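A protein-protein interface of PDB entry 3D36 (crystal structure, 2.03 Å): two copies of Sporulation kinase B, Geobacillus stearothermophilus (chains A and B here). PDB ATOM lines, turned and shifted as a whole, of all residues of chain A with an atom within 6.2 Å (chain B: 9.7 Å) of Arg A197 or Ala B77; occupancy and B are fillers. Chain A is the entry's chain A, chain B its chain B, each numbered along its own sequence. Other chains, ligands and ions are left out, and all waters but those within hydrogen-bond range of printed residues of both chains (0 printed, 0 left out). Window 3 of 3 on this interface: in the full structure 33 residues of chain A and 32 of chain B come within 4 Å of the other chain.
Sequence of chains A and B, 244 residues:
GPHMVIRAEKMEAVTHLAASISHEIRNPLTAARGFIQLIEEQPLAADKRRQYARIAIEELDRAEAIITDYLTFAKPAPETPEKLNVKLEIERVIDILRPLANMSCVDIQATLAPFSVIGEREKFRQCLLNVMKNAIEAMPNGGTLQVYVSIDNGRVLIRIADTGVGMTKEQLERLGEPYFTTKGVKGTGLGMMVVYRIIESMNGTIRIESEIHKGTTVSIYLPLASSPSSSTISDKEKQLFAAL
Printed residues of chain A within 4 Å of Ala B77: Arg A197 (3.5 Å).
No residue of chain B comes within 4 Å of Ile A198.
Of the printed residues of chain B, Ser A201 touches Pro B78.
Printed residues of chain A within 4 Å of Pro B78: Arg A197 and Ser A201.
Printed residues of chain A within 4 Å of Pro B76: Met A193 and Val A194.
Met A202 touches none of the printed residues of chain B.
Lys B75 touches none of the printed residues of chain A.
The backbone carbonyl oxygen (O) of Ile A198 lies within hydrogen-bond range of the side-chain hydroxyl (OG) of Ser A201.
The guanidinium group (NH2) of Arg A197 sits at hydrogen-bond distance from the side-chain sulfur (SD) of Met A193 (3.6 Å).
Among the printed residues, merely in contact across the chains: Arg A197 with Ala B77 (3.5 Å), Arg A197 with Pro B78 (3.8 Å), Ser A201 with Pro B78 (3.9 Å), Val A194 with Pro B76 (3.9 Å) and Met A193 with Pro B76 (3.95 Å).
Of the 14 printed residues of chain A, 4 touch a printed residue of chain B.
Printed residues of chain A that touch a printed residue of chain B: Met A193, Val A194, Arg A197 and Ser A201.
Hydrophobic or aromatic side chains of chain B within 4 Å of the printed part of chain A: Pro B76, Ala B77 and Pro B78.
Among the printed residues, 5 pairs touch across the chains.
No position is printed for both chains.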
ATOM      1  N   LEU A  17      27.468 -25.849   9.894  1.00  0.00           N
ATOM      2  CA  LEU A  17      26.700 -24.648  10.226  1.00  0.00           C
ATOM      3  C   LEU A  17      26.989 -24.130  11.630  1.00  0.00           C
ATOM      4  O   LEU A  17      26.894 -24.868  12.611  1.00  0.00           O
ATOM      5  CB  LEU A  17      25.197 -24.904  10.076  1.00  0.00           C
ATOM      6  CG  LEU A  17      24.557 -24.675   8.706  1.00  0.00           C
ATOM      7  CD1 LEU A  17      23.301 -25.527   8.562  1.00  0.00           C
ATOM      8  CD2 LEU A  17      24.250 -23.189   8.482  1.00  0.00           C
ATOM      9  N   ALA A  18      27.333 -22.851  11.723  1.00  0.00           N
ATOM     10  CA  ALA A  18      27.531 -22.221  13.019  1.00  0.00           C
ATOM     11  C   ALA A  18      26.213 -21.636  13.516  1.00  0.00           C
ATOM     12  O   ALA A  18      25.391 -21.176  12.723  1.00  0.00           O
ATOM     13  CB  ALA A  18      28.590 -21.151  12.928  1.00  0.00           C
ATOM     14  N   PRO A 178      33.472 -25.156  11.382  1.00  0.00           N
ATOM     15  CA  PRO A 178      32.874 -24.659  12.619  1.00  0.00           C
ATOM     16  C   PRO A 178      33.007 -25.671  13.756  1.00  0.00           C
ATOM     17  O   PRO A 178      32.728 -26.862  13.570  1.00  0.00           O
ATOM     18  CB  PRO A 178      31.404 -24.440  12.241  1.00  0.00           C
ATOM     19  CG  PRO A 178      31.422 -24.258  10.762  1.00  0.00           C
ATOM     20  CD  PRO A 178      32.488 -25.197  10.284  1.00  0.00           C
ATOM     21  N   MET A 192      38.751 -19.047  12.912  1.00  0.00           N
ATOM     22  CA  MET A 192      39.159 -19.127  11.513  1.00  0.00           C
ATOM     23  C   MET A 192      37.982 -19.108  10.543  1.00  0.00           C
ATOM     24  O   MET A 192      38.095 -18.575   9.440  1.00  0.00           O
ATOM     25  CB  MET A 192      40.055 -20.339  11.263  1.00  0.00           C
ATOM     26  CG  MET A 192      41.533 -20.028  11.401  1.00  0.00           C
ATOM     27  SD  MET A 192      42.109 -18.677  10.339  1.00  0.00           S
ATOM     28  CE  MET A 192      41.533 -19.200   8.738  1.00  0.00           C
ATOM     29  N   MET A 193      36.857 -19.680  10.964  1.00  0.00           N
ATOM     30  CA  MET A 193      35.621 -19.655  10.183  1.00  0.00           C
ATOM     31  C   MET A 193      35.207 -18.230   9.787  1.00  0.00           C
ATOM     32  O   MET A 193      34.818 -17.983   8.644  1.00  0.00           O
ATOM     33  CB  MET A 193      34.493 -20.321  10.969  1.00  0.00           C
ATOM     34  CG  MET A 193      33.155 -20.337  10.248  1.00  0.00           C
ATOM     35  SD  MET A 193      31.780 -20.661  11.366  1.00  0.00           S
ATOM     36  CE  MET A 193      31.741 -19.153  12.346  1.00  0.00           C
ATOM     37  N   VAL A 194      35.277 -17.297  10.733  1.00  0.00           N
ATOM     38  CA  VAL A 194      34.931 -15.912  10.419  1.00  0.00           C
ATOM     39  C   VAL A 194      36.009 -15.225   9.576  1.00  0.00           C
ATOM     40  O   VAL A 194      35.693 -14.362   8.768  1.00  0.00           O
ATOM     41  CB  VAL A 194      34.546 -15.072  11.666  1.00  0.00           C
ATOM     42  CG1 VAL A 194      33.324 -15.665  12.340  1.00  0.00           C
ATOM     43  CG2 VAL A 194      35.697 -14.970  12.640  1.00  0.00           C
ATOM     44  N   VAL A 195      37.270 -15.620   9.759  1.00  0.00           N
ATOM     45  CA  VAL A 195      38.358 -15.163   8.882  1.00  0.00           C
ATOM     46  C   VAL A 195      38.004 -15.440   7.416  1.00  0.00           C
ATOM     47  O   VAL A 195      38.084 -14.536   6.574  1.00  0.00           O
ATOM     48  CB  VAL A 195      39.726 -15.810   9.242  1.00  0.00           C
ATOM     49  CG1 VAL A 195      40.780 -15.519   8.169  1.00  0.00           C
ATOM     50  CG2 VAL A 195      40.210 -15.325  10.588  1.00  0.00           C
ATOM     51  N   TYR A 196      37.596 -16.677   7.127  1.00  0.00           N
ATOM     52  CA  TYR A 196      37.220 -17.078   5.769  1.00  0.00           C
ATOM     53  C   TYR A 196      36.072 -16.228   5.226  1.00  0.00           C
ATOM     54  O   TYR A 196      36.154 -15.712   4.111  1.00  0.00           O
ATOM     55  CB  TYR A 196      36.821 -18.558   5.708  1.00  0.00           C
ATOM     56  CG  TYR A 196      37.940 -19.559   5.916  1.00  0.00           C
ATOM     57  CD1 TYR A 196      37.653 -20.870   6.287  1.00  0.00           C
ATOM     58  CD2 TYR A 196      39.277 -19.205   5.740  1.00  0.00           C
ATOM     59  CE1 TYR A 196      38.661 -21.801   6.474  1.00  0.00           C
ATOM     60  CE2 TYR A 196      40.295 -20.134   5.922  1.00  0.00           C
ATOM     61  CZ  TYR A 196      39.979 -21.427   6.297  1.00  0.00           C
ATOM     62  OH  TYR A 196      40.976 -22.354   6.484  1.00  0.00           O
ATOM     63  N   ARG A 197      35.015 -16.100   6.026  1.00  0.00           N
ATOM     64  CA  ARG A 197      33.812 -15.352   5.648  1.00  0.00           C
ATOM     65  C   ARG A 197      34.124 -13.884   5.361  1.00  0.00           C
ATOM     66  O   ARG A 197      33.631 -13.332   4.380  1.00  0.00           O
ATOM     67  CB  ARG A 197      32.732 -15.462   6.734  1.00  0.00           C
ATOM     68  CG  ARG A 197      32.404 -16.892   7.187  1.00  0.00           C
ATOM     69  CD  ARG A 197      31.161 -17.458   6.517  1.00  0.00           C
ATOM     70  NE  ARG A 197      30.884 -18.841   6.927  1.00  0.00           N
ATOM     71  CZ  ARG A 197      30.148 -19.202   7.980  1.00  0.00           C
ATOM     72  NH1 ARG A 197      29.596 -18.294   8.778  1.00  0.00           N
ATOM     73  NH2 ARG A 197      29.966 -20.490   8.243  1.00  0.00           N
ATOM     74  N   ILE A 198      34.947 -13.263   6.209  1.00  0.00           N
ATOM     75  CA  ILE A 198      35.342 -11.861   6.019  1.00  0.00           C
ATOM     76  C   ILE A 198      36.191 -11.691   4.750  1.00  0.00           C
ATOM     77  O   ILE A 198      35.943 -10.783   3.956  1.00  0.00           O
ATOM     78  CB  ILE A 198      36.071 -11.276   7.258  1.00  0.00           C
ATOM     79  CG1 ILE A 198      35.116 -11.211   8.457  1.00  0.00           C
ATOM     80  CG2 ILE A 198      36.612  -9.869   6.969  1.00  0.00           C
ATOM     81  CD1 ILE A 198      35.814 -11.258   9.808  1.00  0.00           C
ATOM     82  N   ILE A 199      37.172 -12.573   4.556  1.00  0.00           N
ATOM     83  CA  ILE A 199      38.029 -12.516   3.358  1.00  0.00           C
ATOM     84  C   ILE A 199      37.212 -12.667   2.077  1.00  0.00           C
ATOM     85  O   ILE A 199      37.408 -11.913   1.120  1.00  0.00           O
ATOM     86  CB  ILE A 199      39.197 -13.545   3.412  1.00  0.00           C
ATOM     87  CG1 ILE A 199      40.206 -13.167   4.505  1.00  0.00           C
ATOM     88  CG2 ILE A 199      39.909 -13.659   2.051  1.00  0.00           C
ATOM     89  CD1 ILE A 199      40.600 -11.683   4.544  1.00  0.00           C
ATOM     90  N   GLU A 200      36.284 -13.622   2.076  1.00  0.00           N
ATOM     91  CA  GLU A 200      35.379 -13.827   0.949  1.00  0.00           C
ATOM     92  C   GLU A 200      34.565 -12.571   0.627  1.00  0.00           C
ATOM     93  O   GLU A 200      34.435 -12.196  -0.541  1.00  0.00           O
ATOM     94  CB  GLU A 200      34.447 -15.013   1.212  1.00  0.00           C
ATOM     95  CG  GLU A 200      33.526 -15.347   0.039  1.00  0.00           C
ATOM     96  CD  GLU A 200      32.700 -16.607   0.256  1.00  0.00           C
ATOM     97  OE1 GLU A 200      31.703 -16.790  -0.476  1.00  0.00           O
ATOM     98  OE2 GLU A 200      33.045 -17.415   1.150  1.00  0.00           O
ATOM     99  N   SER A 201      34.036 -11.923   1.665  1.00  0.00           N
ATOM    100  CA  SER A 201      33.196 -10.735   1.499  1.00  0.00           C
ATOM    101  C   SER A 201      33.977  -9.552   0.930  1.00  0.00           C
ATOM    102  O   SER A 201      33.393  -8.647   0.331  1.00  0.00           O
ATOM    103  CB  SER A 201      32.529 -10.350   2.825  1.00  0.00           C
ATOM    104  OG  SER A 201      33.451  -9.728   3.706  1.00  0.00           O
ATOM    105  N   MET A 202      35.295  -9.572   1.118  1.00  0.00           N
ATOM    106  CA  MET A 202      36.190  -8.534   0.611  1.00  0.00           C
ATOM    107  C   MET A 202      36.749  -8.898  -0.767  1.00  0.00           C
ATOM    108  O   MET A 202      37.684  -8.255  -1.260  1.00  0.00           O
ATOM    109  CB  MET A 202      37.333  -8.295   1.601  1.00  0.00           C
ATOM    110  CG  MET A 202      36.887  -7.756   2.965  1.00  0.00           C
ATOM    111  SD  MET A 202      38.257  -7.599   4.127  1.00  0.00           S
ATOM    112  CE  MET A 202      39.247  -6.332   3.325  1.00  0.00           C
ATOM    113  N   PHE B  73      19.543 -11.415  16.281  1.00  0.00           N
ATOM    114  CA  PHE B  73      19.506 -12.126  15.001  1.00  0.00           C
ATOM    115  C   PHE B  73      20.878 -12.255  14.337  1.00  0.00           C
ATOM    116  O   PHE B  73      21.051 -13.073  13.434  1.00  0.00           O
ATOM    117  CB  PHE B  73      18.524 -11.428  14.037  1.00  0.00           C
ATOM    118  CG  PHE B  73      17.136 -11.270  14.600  1.00  0.00           C
ATOM    119  CD1 PHE B  73      16.758 -10.089  15.241  1.00  0.00           C
ATOM    120  CD2 PHE B  73      16.214 -12.310  14.510  1.00  0.00           C
ATOM    121  CE1 PHE B  73      15.482  -9.945  15.772  1.00  0.00           C
ATOM    122  CE2 PHE B  73      14.938 -12.173  15.030  1.00  0.00           C
ATOM    123  CZ  PHE B  73      14.566 -10.983  15.666  1.00  0.00           C
ATOM    124  N   ALA B  74      21.839 -11.443  14.776  1.00  0.00           N
ATOM    125  CA  ALA B  74      23.152 -11.365  14.128  1.00  0.00           C
ATOM    126  C   ALA B  74      23.806 -12.734  13.994  1.00  0.00           C
ATOM    127  O   ALA B  74      23.844 -13.513  14.950  1.00  0.00           O
ATOM    128  CB  ALA B  74      24.074 -10.406  14.878  1.00  0.00           C
ATOM    129  N   LYS B  75      24.292 -13.024  12.791  1.00  0.00           N
ATOM    130  CA  LYS B  75      24.997 -14.269  12.523  1.00  0.00           C
ATOM    131  C   LYS B  75      26.479 -13.970  12.291  1.00  0.00           C
ATOM    132  O   LYS B  75      26.830 -12.852  11.908  1.00  0.00           O
ATOM    133  CB  LYS B  75      24.372 -14.986  11.325  1.00  0.00           C
ATOM    134  CG  LYS B  75      22.961 -15.495  11.587  1.00  0.00           C
ATOM    135  CD  LYS B  75      22.392 -16.175  10.343  1.00  0.00           C
ATOM    136  CE  LYS B  75      20.878 -16.376  10.442  1.00  0.00           C
ATOM    137  NZ  LYS B  75      20.477 -17.263  11.576  1.00  0.00           N
ATOM    138  N   PRO B  76      27.365 -14.956  12.546  1.00  0.00           N
ATOM    139  CA  PRO B  76      28.788 -14.637  12.396  1.00  0.00           C
ATOM    140  C   PRO B  76      29.210 -14.216  10.968  1.00  0.00           C
ATOM    141  O   PRO B  76      30.138 -13.416  10.814  1.00  0.00           O
ATOM    142  CB  PRO B  76      29.503 -15.905  12.890  1.00  0.00           C
ATOM    143  CG  PRO B  76      28.474 -16.989  12.876  1.00  0.00           C
ATOM    144  CD  PRO B  76      27.137 -16.341  13.014  1.00  0.00           C
ATOM    145  N   ALA B  77      28.508 -14.687   9.940  1.00  0.00           N
ATOM    146  CA  ALA B  77      28.811 -14.283   8.556  1.00  0.00           C
ATOM    147  C   ALA B  77      28.349 -12.852   8.203  1.00  0.00           C
ATOM    148  O   ALA B  77      27.197 -12.484   8.469  1.00  0.00           O
ATOM    149  CB  ALA B  77      28.236 -15.293   7.570  1.00  0.00           C
ATOM    150  N   PRO B  78      29.249 -12.039   7.603  1.00  0.00           N
ATOM    151  CA  PRO B  78      28.873 -10.692   7.160  1.00  0.00           C
ATOM    152  C   PRO B  78      27.681 -10.731   6.210  1.00  0.00           C
ATOM    153  O   PRO B  78      27.630 -11.566   5.304  1.00  0.00           O
ATOM    154  CB  PRO B  78      30.130 -10.184   6.436  1.00  0.00           C
ATOM    155  CG  PRO B  78      30.972 -11.386   6.199  1.00  0.00           C
ATOM    156  CD  PRO B  78      30.662 -12.330   7.308  1.00  0.00           C
ATOM    157  N   GLU B  79      26.730  -9.836   6.445  1.00  0.00           N
ATOM    158  CA  GLU B  79      25.464  -9.803   5.721  1.00  0.00           C
ATOM    159  C   GLU B  79      25.588  -9.187   4.339  1.00  0.00           C
ATOM    160  O   GLU B  79      26.428  -8.318   4.111  1.00  0.00           O
ATOM    161  CB  GLU B  79      24.426  -9.006   6.517  1.00  0.00           C
ATOM    162  CG  GLU B  79      23.876  -9.728   7.720  1.00  0.00           C
ATOM    163  CD  GLU B  79      22.536  -9.184   8.157  1.00  0.00           C
ATOM    164  OE1 GLU B  79      22.508  -8.200   8.927  1.00  0.00           O
ATOM    165  OE2 GLU B  79      21.507  -9.747   7.734  1.00  0.00           O
ATOM    166  N   THR B  80      24.733  -9.643   3.428  1.00  0.00           N
ATOM    167  CA  THR B  80      24.563  -9.030   2.115  1.00  0.00           C
ATOM    168  C   THR B  80      23.123  -8.519   2.013  1.00  0.00           C
ATOM    169  O   THR B  80      22.202  -9.201   2.470  1.00  0.00           O
ATOM    170  CB  THR B  80      24.837 -10.050   0.987  1.00  0.00           C
ATOM    171  OG1 THR B  80      26.111 -10.668   1.200  1.00  0.00           O
ATOM    172  CG2 THR B  80      24.835  -9.383  -0.381  1.00  0.00           C
ATOM    173  N   GLU B  82      19.458  -7.938   0.702  1.00  0.00           N
ATOM    174  CA  GLU B  82      18.550  -8.810  -0.046  1.00  0.00           C
ATOM    175  C   GLU B  82      17.182  -8.164  -0.212  1.00  0.00           C
ATOM    176  O   GLU B  82      16.864  -7.169   0.448  1.00  0.00           O
ATOM    177  CB  GLU B  82      18.357 -10.142   0.680  1.00  0.00           C
ATOM    178  CG  GLU B  82      19.602 -10.980   0.863  1.00  0.00           C
ATOM    179  CD  GLU B  82      19.338 -12.191   1.729  1.00  0.00           C
ATOM    180  OE1 GLU B  82      18.632 -13.114   1.268  1.00  0.00           O
ATOM    181  OE2 GLU B  82      19.827 -12.219   2.875  1.00  0.00           O
ATOM    182  N   GLU B 120      19.438  -5.695   4.949  1.00  0.00           N
ATOM    183  CA  GLU B 120      20.100  -6.841   5.546  1.00  0.00           C
ATOM    184  C   GLU B 120      19.184  -7.464   6.594  1.00  0.00           C
ATOM    185  O   GLU B 120      18.799  -6.815   7.562  1.00  0.00           O
ATOM    186  CB  GLU B 120      21.473  -6.434   6.093  1.00  0.00           C
ATOM    187  CG  GLU B 120      22.497  -6.288   4.953  1.00  0.00           C
ATOM    188  CD  GLU B 120      23.754  -5.504   5.303  1.00  0.00           C
ATOM    189  OE1 GLU B 120      24.104  -5.376   6.492  1.00  0.00           O
ATOM    190  OE2 GLU B 120      24.416  -5.028   4.355  1.00  0.00           O
ATOM    191  N   ARG B 121      18.828  -8.727   6.357  1.00  0.00           N
ATOM    192  CA  ARG B 121      17.778  -9.438   7.093  1.00  0.00           C
ATOM    193  C   ARG B 121      17.885  -9.369   8.627  1.00  0.00           C
ATOM    194  O   ARG B 121      16.919  -9.004   9.303  1.00  0.00           O
ATOM    195  CB  ARG B 121      17.732 -10.897   6.631  1.00  0.00           C
ATOM    196  CG  ARG B 121      16.565 -11.706   7.176  1.00  0.00           C
ATOM    197  CD  ARG B 121      16.554 -13.118   6.587  1.00  0.00           C
ATOM    198  NE  ARG B 121      16.607 -13.109   5.122  1.00  0.00           N
ATOM    199  CZ  ARG B 121      15.551 -12.936   4.332  1.00  0.00           C
ATOM    200  NH1 ARG B 121      14.347 -12.759   4.860  1.00  0.00           N
ATOM    201  NH2 ARG B 121      15.696 -12.935   3.016  1.00  0.00           N
ATOM    202  N   GLU B 122      19.053  -9.727   9.158  1.00  0.00           N
ATOM    203  CA  GLU B 122      19.276  -9.780  10.610  1.00  0.00           C
ATOM    204  C   GLU B 122      19.069  -8.401  11.248  1.00  0.00           C
ATOM    205  O   GLU B 122      18.381  -8.273  12.269  1.00  0.00           O
ATOM    206  CB  GLU B 122      20.675 -10.331  10.922  1.00  0.00           C
ATOM    207  CG  GLU B 122      20.944 -11.730  10.353  1.00  0.00           C
ATOM    208  CD  GLU B 122      22.418 -11.996  10.040  1.00  0.00           C
ATOM    209  OE1 GLU B 122      23.312 -11.331  10.615  1.00  0.00           O
ATOM    210  OE2 GLU B 122      22.685 -12.885   9.207  1.00  0.00           O
ATOM    211  N   LYS B 123      19.651  -7.377  10.622  1.00  0.00           N
ATOM    212  CA  LYS B 123      19.558  -6.001  11.094  1.00  0.00           C
ATOM    213  C   LYS B 123      18.129  -5.477  11.036  1.00  0.00           C
ATOM    214  O   LYS B 123      17.677  -4.802  11.960  1.00  0.00           O
ATOM    215  CB  LYS B 123      20.489  -5.087  10.290  1.00  0.00           C
ATOM    216  CG  LYS B 123      21.960  -5.363  10.536  1.00  0.00           C
ATOM    217  CD  LYS B 123      22.846  -4.395   9.774  1.00  0.00           C
ATOM    218  CE  LYS B 123      24.307  -4.781   9.933  1.00  0.00           C
ATOM    219  NZ  LYS B 123      24.673  -5.935   9.072  1.00  0.00           N
